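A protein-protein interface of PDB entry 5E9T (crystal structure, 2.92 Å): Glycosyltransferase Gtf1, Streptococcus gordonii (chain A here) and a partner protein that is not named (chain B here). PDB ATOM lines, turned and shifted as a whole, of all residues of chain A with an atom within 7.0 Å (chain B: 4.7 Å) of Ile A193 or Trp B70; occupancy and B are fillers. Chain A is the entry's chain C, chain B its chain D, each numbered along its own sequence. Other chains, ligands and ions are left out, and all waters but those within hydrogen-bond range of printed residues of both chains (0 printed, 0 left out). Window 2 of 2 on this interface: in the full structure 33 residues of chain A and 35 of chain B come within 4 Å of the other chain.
Of the 10 printed residues of chain A, 5 touch a printed residue of chain B.
Among the printed residues, no Asp or Glu carboxylate lies within 4 Å of a Lys or Arg side-chain nitrogen of the other chain.
The guanidinium group (NH2) of Arg A188 sits close to the indole nitrogen (NE1) of Trp B107.
Trp B70 touches just one residue of chain A: Ile A193.
Of the printed residues of chain B, Arg A192 touches Pro B68.
Printed residues of chain B within 4 Å of Arg A188: Trp B107.
Of the printed residues of chain A, Trp B107 touches Arg A188 and Ile A193.
The nearest residue of chain B that does not touch Ile A193 is Pro B67 (4.1 Å).
NH1 of Arg A188 lies within hydrogen-bond range of O of Pro A190 (3.3 Å).
The guanidinium group of Arg A188 lies within hydrogen-bond range of the backbone carbonyl oxygen of Arg A192 (3.1 Å).
The side-chain carboxylate of Asp A191 lies within salt-bridge range of the guanidinium group of Arg A192.
The indole nitrogen of Trp B70 lies close to the side-chain carboxylate of Asp B83 (3.4 Å).
The backbone carbonyl oxygen of Val B81 lies within hydrogen-bond range of the backbone NH of Arg B88 (2.9 Å).
Asp A191 touches Pro B67.
Pro B68 touches Arg A192.
CG2 of Ile A193 touches CH2 of Trp B70, 3.5 Å away.
Ile A193 touches Trp B107.
OH of Tyr A195 touches CD of Arg B88 (3.6 Å).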
ATOM      1  N   LEU A 186      -7.121 -13.209  -2.864  1.00  0.00           N
ATOM      2  CA  LEU A 186      -7.578 -13.116  -4.244  1.00  0.00           C
ATOM      3  C   LEU A 186      -8.939 -13.783  -4.352  1.00  0.00           C
ATOM      4  O   LEU A 186      -9.167 -14.835  -3.754  1.00  0.00           O
ATOM      5  CB  LEU A 186      -6.577 -13.764  -5.216  1.00  0.00           C
ATOM      6  CG  LEU A 186      -6.665 -13.502  -6.729  1.00  0.00           C
ATOM      7  CD1 LEU A 186      -5.339 -13.832  -7.393  1.00  0.00           C
ATOM      8  CD2 LEU A 186      -7.781 -14.289  -7.406  1.00  0.00           C
ATOM      9  N   TYR A 187      -9.823 -13.184  -5.141  1.00  0.00           N
ATOM     10  CA  TYR A 187     -11.124 -13.760  -5.442  1.00  0.00           C
ATOM     11  C   TYR A 187     -11.278 -13.798  -6.952  1.00  0.00           C
ATOM     12  O   TYR A 187     -11.086 -12.776  -7.620  1.00  0.00           O
ATOM     13  CB  TYR A 187     -12.263 -12.952  -4.816  1.00  0.00           C
ATOM     14  CG  TYR A 187     -12.106 -12.688  -3.335  1.00  0.00           C
ATOM     15  CD1 TYR A 187     -12.392 -13.674  -2.399  1.00  0.00           C
ATOM     16  CD2 TYR A 187     -11.690 -11.447  -2.873  1.00  0.00           C
ATOM     17  CE1 TYR A 187     -12.256 -13.434  -1.045  1.00  0.00           C
ATOM     18  CE2 TYR A 187     -11.552 -11.197  -1.521  1.00  0.00           C
ATOM     19  CZ  TYR A 187     -11.839 -12.192  -0.611  1.00  0.00           C
ATOM     20  OH  TYR A 187     -11.707 -11.940   0.735  1.00  0.00           O
ATOM     21  N   ARG A 188     -11.612 -14.967  -7.493  1.00  0.00           N
ATOM     22  CA  ARG A 188     -11.718 -15.148  -8.937  1.00  0.00           C
ATOM     23  C   ARG A 188     -13.139 -15.569  -9.285  1.00  0.00           C
ATOM     24  O   ARG A 188     -13.584 -16.654  -8.898  1.00  0.00           O
ATOM     25  CB  ARG A 188     -10.702 -16.168  -9.443  1.00  0.00           C
ATOM     26  CG  ARG A 188     -10.757 -16.401 -10.945  1.00  0.00           C
ATOM     27  CD  ARG A 188     -10.805 -15.098 -11.731  1.00  0.00           C
ATOM     28  NE  ARG A 188     -10.366 -15.273 -13.114  1.00  0.00           N
ATOM     29  CZ  ARG A 188     -10.850 -14.593 -14.150  1.00  0.00           C
ATOM     30  NH1 ARG A 188     -11.810 -13.695 -13.973  1.00  0.00           N
ATOM     31  NH2 ARG A 188     -10.381 -14.820 -15.368  1.00  0.00           N
ATOM     32  N   PHE A 189     -13.842 -14.707 -10.007  1.00  0.00           N
ATOM     33  CA  PHE A 189     -15.151 -15.014 -10.560  1.00  0.00           C
ATOM     34  C   PHE A 189     -14.953 -15.399 -12.021  1.00  0.00           C
ATOM     35  O   PHE A 189     -13.822 -15.338 -12.519  1.00  0.00           O
ATOM     36  CB  PHE A 189     -16.087 -13.810 -10.431  1.00  0.00           C
ATOM     37  CG  PHE A 189     -16.558 -13.551  -9.028  1.00  0.00           C
ATOM     38  CD1 PHE A 189     -15.658 -13.237  -8.022  1.00  0.00           C
ATOM     39  CD2 PHE A 189     -17.907 -13.603  -8.719  1.00  0.00           C
ATOM     40  CE1 PHE A 189     -16.093 -12.996  -6.734  1.00  0.00           C
ATOM     41  CE2 PHE A 189     -18.349 -13.359  -7.433  1.00  0.00           C
ATOM     42  CZ  PHE A 189     -17.440 -13.055  -6.438  1.00  0.00           C
ATOM     43  N   PRO A 190     -15.999 -15.803 -12.745  1.00  0.00           N
ATOM     44  CA  PRO A 190     -15.830 -15.934 -14.200  1.00  0.00           C
ATOM     45  C   PRO A 190     -15.461 -14.619 -14.867  1.00  0.00           C
ATOM     46  O   PRO A 190     -14.538 -14.582 -15.691  1.00  0.00           O
ATOM     47  CB  PRO A 190     -17.196 -16.461 -14.659  1.00  0.00           C
ATOM     48  CG  PRO A 190     -17.723 -17.195 -13.479  1.00  0.00           C
ATOM     49  CD  PRO A 190     -17.252 -16.427 -12.278  1.00  0.00           C
ATOM     50  N   ASP A 191     -16.176 -13.537 -14.554  1.00  0.00           N
ATOM     51  CA  ASP A 191     -15.917 -12.227 -15.142  1.00  0.00           C
ATOM     52  C   ASP A 191     -15.194 -11.226 -14.239  1.00  0.00           C
ATOM     53  O   ASP A 191     -15.024 -10.076 -14.652  1.00  0.00           O
ATOM     54  CB  ASP A 191     -17.229 -11.613 -15.649  1.00  0.00           C
ATOM     55  CG  ASP A 191     -18.308 -11.590 -14.596  1.00  0.00           C
ATOM     56  OD1 ASP A 191     -18.252 -12.421 -13.664  1.00  0.00           O
ATOM     57  OD2 ASP A 191     -19.222 -10.747 -14.709  1.00  0.00           O
ATOM     58  N   ARG A 192     -14.793 -11.592 -13.018  1.00  0.00           N
ATOM     59  CA  ARG A 192     -14.157 -10.631 -12.118  1.00  0.00           C
ATOM     60  C   ARG A 192     -12.916 -11.219 -11.462  1.00  0.00           C
ATOM     61  O   ARG A 192     -12.806 -12.434 -11.279  1.00  0.00           O
ATOM     62  CB  ARG A 192     -15.106 -10.164 -11.000  1.00  0.00           C
ATOM     63  CG  ARG A 192     -16.349  -9.440 -11.461  1.00  0.00           C
ATOM     64  CD  ARG A 192     -16.021  -8.219 -12.289  1.00  0.00           C
ATOM     65  NE  ARG A 192     -17.170  -7.816 -13.092  1.00  0.00           N
ATOM     66  CZ  ARG A 192     -18.007  -6.837 -12.766  1.00  0.00           C
ATOM     67  NH1 ARG A 192     -17.823  -6.141 -11.651  1.00  0.00           N
ATOM     68  NH2 ARG A 192     -19.028  -6.551 -13.561  1.00  0.00           N
ATOM     69  N   ILE A 193     -11.988 -10.337 -11.089  1.00  0.00           N
ATOM     70  CA  ILE A 193     -10.878 -10.689 -10.207  1.00  0.00           C
ATOM     71  C   ILE A 193     -10.710  -9.565  -9.189  1.00  0.00           C
ATOM     72  O   ILE A 193     -10.802  -8.382  -9.532  1.00  0.00           O
ATOM     73  CB  ILE A 193      -9.571 -10.965 -10.990  1.00  0.00           C
ATOM     74  CG1 ILE A 193      -8.590 -11.766 -10.130  1.00  0.00           C
ATOM     75  CG2 ILE A 193      -8.920  -9.679 -11.477  1.00  0.00           C
ATOM     76  CD1 ILE A 193      -7.359 -12.228 -10.876  1.00  0.00           C
ATOM     77  N   PHE A 194     -10.509  -9.944  -7.923  1.00  0.00           N
ATOM     78  CA  PHE A 194     -10.446  -9.006  -6.808  1.00  0.00           C
ATOM     79  C   PHE A 194      -9.308  -9.391  -5.876  1.00  0.00           C
ATOM     80  O   PHE A 194      -9.090 -10.576  -5.608  1.00  0.00           O
ATOM     81  CB  PHE A 194     -11.751  -8.975  -6.012  1.00  0.00           C
ATOM     82  CG  PHE A 194     -12.922  -8.443  -6.774  1.00  0.00           C
ATOM     83  CD1 PHE A 194     -12.954  -7.129  -7.196  1.00  0.00           C
ATOM     84  CD2 PHE A 194     -14.010  -9.254  -7.042  1.00  0.00           C
ATOM     85  CE1 PHE A 194     -14.043  -6.637  -7.885  1.00  0.00           C
ATOM     86  CE2 PHE A 194     -15.100  -8.768  -7.730  1.00  0.00           C
ATOM     87  CZ  PHE A 194     -15.117  -7.457  -8.154  1.00  0.00           C
ATOM     88  N   TYR A 195      -8.558  -8.388  -5.424  1.00  0.00           N
ATOM     89  CA  TYR A 195      -7.365  -8.602  -4.615  1.00  0.00           C
ATOM     90  C   TYR A 195      -7.521  -8.310  -3.123  1.00  0.00           C
ATOM     91  O   TYR A 195      -6.540  -8.449  -2.383  1.00  0.00           O
ATOM     92  CB  TYR A 195      -6.219  -7.791  -5.218  1.00  0.00           C
ATOM     93  CG  TYR A 195      -6.021  -8.179  -6.662  1.00  0.00           C
ATOM     94  CD1 TYR A 195      -5.277  -9.300  -6.996  1.00  0.00           C
ATOM     95  CD2 TYR A 195      -6.627  -7.464  -7.688  1.00  0.00           C
ATOM     96  CE1 TYR A 195      -5.113  -9.681  -8.309  1.00  0.00           C
ATOM     97  CE2 TYR A 195      -6.464  -7.838  -9.009  1.00  0.00           C
ATOM     98  CZ  TYR A 195      -5.702  -8.946  -9.313  1.00  0.00           C
ATOM     99  OH  TYR A 195      -5.532  -9.326 -10.624  1.00  0.00           O
ATOM    100  N   VAL B  66     -12.437 -10.563 -19.624  1.00  0.00           N
ATOM    101  CA  VAL B  66     -11.736  -9.782 -18.606  1.00  0.00           C
ATOM    102  C   VAL B  66     -12.745  -8.871 -17.923  1.00  0.00           C
ATOM    103  O   VAL B  66     -13.822  -8.594 -18.475  1.00  0.00           O
ATOM    104  CB  VAL B  66     -10.568  -8.968 -19.214  1.00  0.00           C
ATOM    105  CG1 VAL B  66      -9.494  -9.892 -19.764  1.00  0.00           C
ATOM    106  CG2 VAL B  66     -11.078  -8.027 -20.288  1.00  0.00           C
ATOM    107  N   PRO B  67     -12.430  -8.395 -16.717  1.00  0.00           N
ATOM    108  CA  PRO B  67     -13.359  -7.518 -15.989  1.00  0.00           C
ATOM    109  C   PRO B  67     -13.764  -6.323 -16.831  1.00  0.00           C
ATOM    110  O   PRO B  67     -13.002  -5.886 -17.708  1.00  0.00           O
ATOM    111  CB  PRO B  67     -12.543  -7.088 -14.764  1.00  0.00           C
ATOM    112  CG  PRO B  67     -11.612  -8.220 -14.537  1.00  0.00           C
ATOM    113  CD  PRO B  67     -11.255  -8.745 -15.897  1.00  0.00           C
ATOM    114  N   PRO B  68     -14.955  -5.772 -16.599  1.00  0.00           N
ATOM    115  CA  PRO B  68     -15.490  -4.746 -17.506  1.00  0.00           C
ATOM    116  C   PRO B  68     -14.542  -3.565 -17.651  1.00  0.00           C
ATOM    117  O   PRO B  68     -14.042  -3.024 -16.663  1.00  0.00           O
ATOM    118  CB  PRO B  68     -16.808  -4.334 -16.839  1.00  0.00           C
ATOM    119  CG  PRO B  68     -17.183  -5.505 -15.987  1.00  0.00           C
ATOM    120  CD  PRO B  68     -15.888  -6.088 -15.505  1.00  0.00           C
ATOM    121  N   PHE B  69     -14.285  -3.190 -18.904  1.00  0.00           N
ATOM    122  CA  PHE B  69     -13.493  -2.061 -19.381  1.00  0.00           C
ATOM    123  C   PHE B  69     -11.989  -2.331 -19.378  1.00  0.00           C
ATOM    124  O   PHE B  69     -11.246  -1.536 -19.958  1.00  0.00           O
ATOM    125  CB  PHE B  69     -13.753  -0.758 -18.600  1.00  0.00           C
ATOM    126  CG  PHE B  69     -15.150  -0.236 -18.741  1.00  0.00           C
ATOM    127  CD1 PHE B  69     -15.515   0.507 -19.853  1.00  0.00           C
ATOM    128  CD2 PHE B  69     -16.096  -0.480 -17.760  1.00  0.00           C
ATOM    129  CE1 PHE B  69     -16.803   0.995 -19.988  1.00  0.00           C
ATOM    130  CE2 PHE B  69     -17.384   0.004 -17.890  1.00  0.00           C
ATOM    131  CZ  PHE B  69     -17.737   0.744 -19.004  1.00  0.00           C
ATOM    132  N   TRP B  70     -11.506  -3.411 -18.765  1.00  0.00           N
ATOM    133  CA  TRP B  70     -10.070  -3.673 -18.763  1.00  0.00           C
ATOM    134  C   TRP B  70      -9.553  -3.833 -20.189  1.00  0.00           C
ATOM    135  O   TRP B  70     -10.247  -4.344 -21.072  1.00  0.00           O
ATOM    136  CB  TRP B  70      -9.744  -4.920 -17.940  1.00  0.00           C
ATOM    137  CG  TRP B  70      -9.953  -4.746 -16.459  1.00  0.00           C
ATOM    138  CD1 TRP B  70     -10.770  -3.841 -15.844  1.00  0.00           C
ATOM    139  CD2 TRP B  70      -9.329  -5.495 -15.409  1.00  0.00           C
ATOM    140  NE1 TRP B  70     -10.699  -3.986 -14.480  1.00  0.00           N
ATOM    141  CE2 TRP B  70      -9.820  -4.994 -14.189  1.00  0.00           C
ATOM    142  CE3 TRP B  70      -8.405  -6.544 -15.383  1.00  0.00           C
ATOM    143  CZ2 TRP B  70      -9.419  -5.504 -12.960  1.00  0.00           C
ATOM    144  CZ3 TRP B  70      -8.008  -7.047 -14.160  1.00  0.00           C
ATOM    145  CH2 TRP B  70      -8.514  -6.528 -12.967  1.00  0.00           C
ATOM    146  N   GLU B  71      -8.323  -3.379 -20.414  1.00  0.00           N
ATOM    147  CA  GLU B  71      -7.752  -3.310 -21.752  1.00  0.00           C
ATOM    148  C   GLU B  71      -6.862  -4.517 -22.017  1.00  0.00           C
ATOM    149  O   GLU B  71      -6.129  -4.973 -21.132  1.00  0.00           O
ATOM    150  CB  GLU B  71      -6.967  -2.004 -21.946  1.00  0.00           C
ATOM    151  CG  GLU B  71      -5.444  -2.107 -21.909  1.00  0.00           C
ATOM    152  CD  GLU B  71      -4.764  -0.801 -22.298  1.00  0.00           C
ATOM    153  OE1 GLU B  71      -3.873  -0.339 -21.550  1.00  0.00           O
ATOM    154  OE2 GLU B  71      -5.122  -0.230 -23.350  1.00  0.00           O
ATOM    155  N   ILE B  72      -6.956  -5.047 -23.234  1.00  0.00           N
ATOM    156  CA  ILE B  72      -6.117  -6.147 -23.691  1.00  0.00           C
ATOM    157  C   ILE B  72      -5.239  -5.628 -24.818  1.00  0.00           C
ATOM    158  O   ILE B  72      -5.744  -5.105 -25.820  1.00  0.00           O
ATOM    159  CB  ILE B  72      -6.946  -7.350 -24.161  1.00  0.00           C
ATOM    160  CG1 ILE B  72      -7.830  -7.877 -23.032  1.00  0.00           C
ATOM    161  CG2 ILE B  72      -6.028  -8.444 -24.674  1.00  0.00           C
ATOM    162  CD1 ILE B  72      -8.555  -9.168 -23.375  1.00  0.00           C
ATOM    163  N   VAL B  81      -3.264  -8.417 -20.045  1.00  0.00           N
ATOM    164  CA  VAL B  81      -4.437  -7.723 -19.528  1.00  0.00           C
ATOM    165  C   VAL B  81      -3.957  -6.649 -18.562  1.00  0.00           C
ATOM    166  O   VAL B  81      -3.032  -6.882 -17.773  1.00  0.00           O
ATOM    167  CB  VAL B  81      -5.415  -8.692 -18.830  1.00  0.00           C
ATOM    168  CG1 VAL B  81      -6.694  -7.971 -18.445  1.00  0.00           C
ATOM    169  CG2 VAL B  81      -5.720  -9.880 -19.722  1.00  0.00           C
ATOM    170  N   SER B  82      -4.579  -5.475 -18.626  1.00  0.00           N
ATOM    171  CA  SER B  82      -4.162  -4.342 -17.816  1.00  0.00           C
ATOM    172  C   SER B  82      -5.380  -3.635 -17.245  1.00  0.00           C
ATOM    173  O   SER B  82      -6.368  -3.419 -17.953  1.00  0.00           O
ATOM    174  CB  SER B  82      -3.333  -3.342 -18.634  1.00  0.00           C
ATOM    175  OG  SER B  82      -2.351  -4.000 -19.414  1.00  0.00           O
ATOM    176  N   ASP B  83      -5.300  -3.275 -15.964  1.00  0.00           N
ATOM    177  CA  ASP B  83      -6.294  -2.435 -15.305  1.00  0.00           C
ATOM    178  C   ASP B  83      -5.667  -1.066 -15.086  1.00  0.00           C
ATOM    179  O   ASP B  83      -4.657  -0.954 -14.382  1.00  0.00           O
ATOM    180  CB  ASP B  83      -6.754  -3.039 -13.976  1.00  0.00           C
ATOM    181  CG  ASP B  83      -7.935  -2.285 -13.359  1.00  0.00           C
ATOM    182  OD1 ASP B  83      -8.380  -1.274 -13.941  1.00  0.00           O
ATOM    183  OD2 ASP B  83      -8.417  -2.700 -12.284  1.00  0.00           O
ATOM    184  N   ARG B  88      -1.873  -7.115 -15.074  1.00  0.00           N
ATOM    185  CA  ARG B  88      -2.768  -7.970 -14.311  1.00  0.00           C
ATOM    186  C   ARG B  88      -2.579  -9.409 -14.776  1.00  0.00           C
ATOM    187  O   ARG B  88      -2.327 -10.300 -13.957  1.00  0.00           O
ATOM    188  CB  ARG B  88      -4.220  -7.505 -14.447  1.00  0.00           C
ATOM    189  CG  ARG B  88      -4.495  -6.176 -13.742  1.00  0.00           C
ATOM    190  CD  ARG B  88      -4.411  -6.312 -12.221  1.00  0.00           C
ATOM    191  NE  ARG B  88      -4.513  -5.024 -11.532  1.00  0.00           N
ATOM    192  CZ  ARG B  88      -3.488  -4.394 -10.962  1.00  0.00           C
ATOM    193  NH1 ARG B  88      -2.278  -4.937 -10.986  1.00  0.00           N
ATOM    194  NH2 ARG B  88      -3.673  -3.228 -10.360  1.00  0.00           N
ATOM    195  N   TRP B 107      -3.041 -14.889 -14.459  1.00  0.00           N
ATOM    196  CA  TRP B 107      -3.413 -13.717 -13.679  1.00  0.00           C
ATOM    197  C   TRP B 107      -2.408 -13.479 -12.557  1.00  0.00           C
ATOM    198  O   TRP B 107      -1.878 -14.423 -11.964  1.00  0.00           O
ATOM    199  CB  TRP B 107      -4.821 -13.875 -13.107  1.00  0.00           C
ATOM    200  CG  TRP B 107      -5.884 -13.910 -14.164  1.00  0.00           C
ATOM    201  CD1 TRP B 107      -6.403 -15.017 -14.764  1.00  0.00           C
ATOM    202  CD2 TRP B 107      -6.552 -12.785 -14.751  1.00  0.00           C
ATOM    203  NE1 TRP B 107      -7.355 -14.653 -15.684  1.00  0.00           N
ATOM    204  CE2 TRP B 107      -7.464 -13.289 -15.697  1.00  0.00           C
ATOM    205  CE3 TRP B 107      -6.468 -11.402 -14.566  1.00  0.00           C
ATOM    206  CZ2 TRP B 107      -8.287 -12.460 -16.458  1.00  0.00           C
ATOM    207  CZ3 TRP B 107      -7.287 -10.578 -15.322  1.00  0.00           C
ATOM    208  CH2 TRP B 107      -8.185 -11.111 -16.258  1.00  0.00           C
